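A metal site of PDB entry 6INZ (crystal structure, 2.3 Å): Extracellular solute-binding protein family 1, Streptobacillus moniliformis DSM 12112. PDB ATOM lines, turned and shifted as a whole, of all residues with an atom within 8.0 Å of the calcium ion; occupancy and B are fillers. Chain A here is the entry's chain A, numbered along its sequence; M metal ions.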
ATOM      1  N   TRP A 163      -4.234   3.964 -19.612  1.00  0.00           N
ATOM      2  CA  TRP A 163      -5.388   4.657 -19.040  1.00  0.00           C
ATOM      3  C   TRP A 163      -5.564   4.295 -17.564  1.00  0.00           C
ATOM      4  O   TRP A 163      -6.038   5.110 -16.775  1.00  0.00           O
ATOM      5  CB  TRP A 163      -6.639   4.328 -19.820  1.00  0.00           C
ATOM      6  CG  TRP A 163      -6.694   5.060 -21.102  1.00  0.00           C
ATOM      7  CD1 TRP A 163      -5.735   5.875 -21.636  1.00  0.00           C
ATOM      8  CD2 TRP A 163      -7.761   5.040 -22.024  1.00  0.00           C
ATOM      9  NE1 TRP A 163      -6.168   6.414 -22.814  1.00  0.00           N
ATOM     10  CE2 TRP A 163      -7.403   5.892 -23.093  1.00  0.00           C
ATOM     11  CE3 TRP A 163      -9.007   4.427 -22.041  1.00  0.00           C
ATOM     12  CZ2 TRP A 163      -8.238   6.090 -24.179  1.00  0.00           C
ATOM     13  CZ3 TRP A 163      -9.828   4.633 -23.110  1.00  0.00           C
ATOM     14  CH2 TRP A 163      -9.451   5.442 -24.156  1.00  0.00           C
ATOM     15  N   PHE A 185     -13.366   4.679 -17.337  1.00  0.00           N
ATOM     16  CA  PHE A 185     -12.896   5.054 -18.670  1.00  0.00           C
ATOM     17  C   PHE A 185     -13.919   5.912 -19.382  1.00  0.00           C
ATOM     18  O   PHE A 185     -13.555   6.821 -20.125  1.00  0.00           O
ATOM     19  CB  PHE A 185     -12.624   3.857 -19.585  1.00  0.00           C
ATOM     20  CG  PHE A 185     -11.397   3.116 -19.265  1.00  0.00           C
ATOM     21  CD1 PHE A 185     -10.544   3.554 -18.280  1.00  0.00           C
ATOM     22  CD2 PHE A 185     -11.098   1.912 -19.956  1.00  0.00           C
ATOM     23  CE1 PHE A 185      -9.404   2.837 -17.987  1.00  0.00           C
ATOM     24  CE2 PHE A 185      -9.959   1.217 -19.671  1.00  0.00           C
ATOM     25  CZ  PHE A 185      -9.094   1.686 -18.680  1.00  0.00           C
ATOM     26  N   ARG A 186     -15.206   5.635 -19.175  1.00  0.00           N
ATOM     27  CA  ARG A 186     -16.209   6.379 -19.929  1.00  0.00           C
ATOM     28  C   ARG A 186     -16.340   7.809 -19.439  1.00  0.00           C
ATOM     29  O   ARG A 186     -16.568   8.710 -20.255  1.00  0.00           O
ATOM     30  CB  ARG A 186     -17.600   5.724 -19.860  1.00  0.00           C
ATOM     31  CG  ARG A 186     -18.489   6.310 -21.008  1.00  0.00           C
ATOM     32  CD  ARG A 186     -19.945   5.978 -20.835  1.00  0.00           C
ATOM     33  NE  ARG A 186     -20.522   6.475 -19.576  1.00  0.00           N
ATOM     34  CZ  ARG A 186     -21.178   7.646 -19.448  1.00  0.00           C
ATOM     35  NH1 ARG A 186     -21.335   8.448 -20.487  1.00  0.00           N
ATOM     36  NH2 ARG A 186     -21.679   8.015 -18.281  1.00  0.00           N
ATOM     37  N   GLU A 187     -16.263   8.013 -18.102  1.00  0.00           N
ATOM     38  CA  GLU A 187     -16.628   9.252 -17.382  1.00  0.00           C
ATOM     39  C   GLU A 187     -15.466  10.200 -17.082  1.00  0.00           C
ATOM     40  O   GLU A 187     -15.702  11.389 -16.975  1.00  0.00           O
ATOM     41  CB  GLU A 187     -17.291   8.908 -16.037  1.00  0.00           C
ATOM     42  CG  GLU A 187     -18.703   8.267 -16.121  1.00  0.00           C
ATOM     43  CD  GLU A 187     -19.218   7.753 -14.713  1.00  0.00           C
ATOM     44  OE1 GLU A 187     -18.393   7.754 -13.742  1.00  0.00           O
ATOM     45  OE2 GLU A 187     -20.394   7.318 -14.600  1.00  0.00           O
ATOM     46  N   LYS A 188     -14.243   9.715 -16.913  1.00  0.00           N
ATOM     47  CA  LYS A 188     -13.136  10.534 -16.396  1.00  0.00           C
ATOM     48  C   LYS A 188     -12.087  10.882 -17.442  1.00  0.00           C
ATOM     49  O   LYS A 188     -10.933  11.079 -17.094  1.00  0.00           O
ATOM     50  CB  LYS A 188     -12.450   9.830 -15.220  1.00  0.00           C
ATOM     51  CG  LYS A 188     -13.410   9.405 -14.071  1.00  0.00           C
ATOM     52  CD  LYS A 188     -14.024  10.631 -13.353  1.00  0.00           C
ATOM     53  CE  LYS A 188     -14.672  10.335 -11.976  1.00  0.00           C
ATOM     54  NZ  LYS A 188     -14.175  11.296 -10.918  1.00  0.00           N
ATOM     55  N   ASP A 189     -12.438  10.893 -18.739  1.00  0.00           N
ATOM     56  CA  ASP A 189     -11.629  11.476 -19.807  1.00  0.00           C
ATOM     57  C   ASP A 189     -10.167  11.033 -19.894  1.00  0.00           C
ATOM     58  O   ASP A 189      -9.274  11.878 -19.977  1.00  0.00           O
ATOM     59  CB  ASP A 189     -11.686  13.000 -19.704  1.00  0.00           C
ATOM     60  CG  ASP A 189     -11.099  13.691 -20.965  1.00  0.00           C
ATOM     61  OD1 ASP A 189     -11.357  13.221 -22.097  1.00  0.00           O
ATOM     62  OD2 ASP A 189     -10.340  14.675 -20.836  1.00  0.00           O
ATOM     63  N   PRO A 190      -9.882   9.718 -19.897  1.00  0.00           N
ATOM     64  CA  PRO A 190      -8.470   9.289 -19.807  1.00  0.00           C
ATOM     65  C   PRO A 190      -7.628   9.706 -21.011  1.00  0.00           C
ATOM     66  O   PRO A 190      -6.400   9.778 -20.907  1.00  0.00           O
ATOM     67  CB  PRO A 190      -8.565   7.750 -19.703  1.00  0.00           C
ATOM     68  CG  PRO A 190      -9.880   7.392 -20.213  1.00  0.00           C
ATOM     69  CD  PRO A 190     -10.786   8.541 -19.896  1.00  0.00           C
ATOM     70  N   ASN A 191      -8.234   9.959 -22.163  1.00  0.00           N
ATOM     71  CA  ASN A 191      -7.462  10.454 -23.269  1.00  0.00           C
ATOM     72  C   ASN A 191      -7.325  11.975 -23.228  1.00  0.00           C
ATOM     73  O   ASN A 191      -6.914  12.561 -24.230  1.00  0.00           O
ATOM     74  CB  ASN A 191      -8.061   9.987 -24.618  1.00  0.00           C
ATOM     75  CG  ASN A 191      -9.330  10.666 -24.974  1.00  0.00           C
ATOM     76  OD1 ASN A 191      -9.719  11.641 -24.374  1.00  0.00           O
ATOM     77  ND2 ASN A 191     -10.022  10.123 -25.996  1.00  0.00           N
ATOM     78  N   GLY A 192      -7.749  12.611 -22.123  1.00  0.00           N
ATOM     79  CA  GLY A 192      -7.338  13.962 -21.760  1.00  0.00           C
ATOM     80  C   GLY A 192      -7.715  15.037 -22.744  1.00  0.00           C
ATOM     81  O   GLY A 192      -7.094  16.111 -22.722  1.00  0.00           O
ATOM     82  N   ASN A 193      -8.683  14.796 -23.612  1.00  0.00           N
ATOM     83  CA  ASN A 193      -9.114  15.794 -24.573  1.00  0.00           C
ATOM     84  C   ASN A 193     -10.329  16.552 -24.092  1.00  0.00           C
ATOM     85  O   ASN A 193     -10.899  17.357 -24.841  1.00  0.00           O
ATOM     86  CB  ASN A 193      -9.362  15.142 -25.975  1.00  0.00           C
ATOM     87  CG  ASN A 193     -10.612  14.203 -26.051  1.00  0.00           C
ATOM     88  OD1 ASN A 193     -11.431  14.143 -25.150  1.00  0.00           O
ATOM     89  ND2 ASN A 193     -10.769  13.527 -27.181  1.00  0.00           N
ATOM     90  N   GLY A 194     -10.797  16.320 -22.862  1.00  0.00           N
ATOM     91  CA  GLY A 194     -11.967  17.055 -22.430  1.00  0.00           C
ATOM     92  C   GLY A 194     -13.281  16.656 -23.073  1.00  0.00           C
ATOM     93  O   GLY A 194     -14.318  17.242 -22.709  1.00  0.00           O
ATOM     94  N   LYS A 195     -13.317  15.657 -23.975  1.00  0.00           N
ATOM     95  CA  LYS A 195     -14.553  15.189 -24.600  1.00  0.00           C
ATOM     96  C   LYS A 195     -14.880  13.776 -24.061  1.00  0.00           C
ATOM     97  O   LYS A 195     -13.961  13.025 -23.746  1.00  0.00           O
ATOM     98  CB  LYS A 195     -14.372  15.256 -26.145  1.00  0.00           C
ATOM     99  CG  LYS A 195     -15.667  15.256 -27.023  1.00  0.00           C
ATOM    100  CD  LYS A 195     -16.475  16.585 -27.176  1.00  0.00           C
ATOM    101  CE  LYS A 195     -17.768  16.438 -28.097  1.00  0.00           C
ATOM    102  NZ  LYS A 195     -19.056  16.028 -27.434  1.00  0.00           N
ATOM    103  N   LYS A 196     -16.189  13.447 -23.879  1.00  0.00           N
ATOM    104  CA  LYS A 196     -16.688  12.106 -23.474  1.00  0.00           C
ATOM    105  C   LYS A 196     -16.864  11.185 -24.700  1.00  0.00           C
ATOM    106  O   LYS A 196     -17.963  10.789 -25.109  1.00  0.00           O
ATOM    107  CB  LYS A 196     -18.018  12.189 -22.707  1.00  0.00           C
ATOM    108  CG  LYS A 196     -17.873  12.186 -21.164  1.00  0.00           C
ATOM    109  CD  LYS A 196     -19.149  12.566 -20.383  1.00  0.00           C
ATOM    110  CE  LYS A 196     -18.823  13.288 -19.026  1.00  0.00           C
ATOM    111  NZ  LYS A 196     -19.930  14.203 -18.545  1.00  0.00           N
ATOM    112  N   ASP A 197     -15.726  10.847 -25.301  1.00  0.00           N
ATOM    113  CA  ASP A 197     -15.692  10.094 -26.534  1.00  0.00           C
ATOM    114  C   ASP A 197     -15.144   8.691 -26.324  1.00  0.00           C
ATOM    115  O   ASP A 197     -15.078   7.908 -27.260  1.00  0.00           O
ATOM    116  CB  ASP A 197     -14.841  10.836 -27.599  1.00  0.00           C
ATOM    117  CG  ASP A 197     -13.387  11.194 -27.072  1.00  0.00           C
ATOM    118  OD1 ASP A 197     -13.080  11.199 -25.850  1.00  0.00           O
ATOM    119  OD2 ASP A 197     -12.510  11.520 -27.875  1.00  0.00           O
ATOM    120  N   GLU A 198     -14.674   8.371 -25.113  1.00  0.00           N
ATOM    121  CA  GLU A 198     -14.021   7.084 -24.935  1.00  0.00           C
ATOM    122  C   GLU A 198     -14.999   5.953 -25.241  1.00  0.00           C
ATOM    123  O   GLU A 198     -16.225   6.071 -25.058  1.00  0.00           O
ATOM    124  CB  GLU A 198     -13.447   6.962 -23.520  1.00  0.00           C
ATOM    125  CG  GLU A 198     -12.097   7.676 -23.420  1.00  0.00           C
ATOM    126  CD  GLU A 198     -12.203   9.209 -23.216  1.00  0.00           C
ATOM    127  OE1 GLU A 198     -13.330   9.739 -23.313  1.00  0.00           O
ATOM    128  OE2 GLU A 198     -11.155   9.865 -22.935  1.00  0.00           O
ATOM    129  N   VAL A 199     -14.453   4.903 -25.828  1.00  0.00           N
ATOM    130  CA  VAL A 199     -15.240   3.711 -26.143  1.00  0.00           C
ATOM    131  C   VAL A 199     -14.630   2.639 -25.266  1.00  0.00           C
ATOM    132  O   VAL A 199     -13.601   2.030 -25.632  1.00  0.00           O
ATOM    133  CB  VAL A 199     -15.192   3.372 -27.626  1.00  0.00           C
ATOM    134  CG1 VAL A 199     -15.889   2.014 -27.862  1.00  0.00           C
ATOM    135  CG2 VAL A 199     -15.914   4.508 -28.347  1.00  0.00           C
ATOM    136  N   ASN A 276      -7.327   6.777 -30.318  1.00  0.00           N
ATOM    137  CA  ASN A 276      -7.212   6.837 -28.865  1.00  0.00           C
ATOM    138  C   ASN A 276      -8.584   6.843 -28.181  1.00  0.00           C
ATOM    139  O   ASN A 276      -8.786   7.538 -27.194  1.00  0.00           O
ATOM    140  CB  ASN A 276      -6.377   8.057 -28.414  1.00  0.00           C
ATOM    141  CG  ASN A 276      -5.798   7.854 -26.990  1.00  0.00           C
ATOM    142  OD1 ASN A 276      -5.693   6.714 -26.531  1.00  0.00           O
ATOM    143  ND2 ASN A 276      -5.399   8.957 -26.309  1.00  0.00           N
ATOM    144  N   LEU A 277      -9.553   6.066 -28.730  1.00  0.00           N
ATOM    145  CA  LEU A 277     -10.910   6.026 -28.181  1.00  0.00           C
ATOM    146  C   LEU A 277     -11.170   4.780 -27.367  1.00  0.00           C
ATOM    147  O   LEU A 277     -12.041   4.801 -26.498  1.00  0.00           O
ATOM    148  CB  LEU A 277     -11.975   6.090 -29.272  1.00  0.00           C
ATOM    149  CG  LEU A 277     -11.901   7.295 -30.193  1.00  0.00           C
ATOM    150  CD1 LEU A 277     -12.817   7.092 -31.370  1.00  0.00           C
ATOM    151  CD2 LEU A 277     -12.275   8.591 -29.419  1.00  0.00           C
HETATM  152 CA    CA M   1     -11.917  12.042 -23.969  1.00  0.00          CA
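Six residues have an atom within 4 Å of the calcium ion: Asp 189, Asn 191, Asn 193, Lys 195, Asp 197 and Glu 198.
The calcium ion is bound by OD1 of Asn 191, 2.3 Å away. O of Lys 195 binds the calcium ion (2.3 Å). The side-chain carboxylate (OD1) of Asp 189 is bound to the calcium ion. OD1 of Asp 197 binds the calcium ion (2.4 Å). The calcium ion is bound by OD1 of Asn 193 (2.5 Å). The calcium ion is bound by OE2 of Glu 198 (2.5 Å). The side-chain carboxylate (OE1) of Glu 198 is bound to the calcium ion, 2.8 Å away.
The side-chain amide nitrogen (ND2) of Asn 191 is in hydrogen-bond range of the backbone carbonyl oxygen (O) of Asn 276. The backbone NH of Gly 194 is in hydrogen-bond range of the side-chain carboxylate of Asp 189 (2.6 Å).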
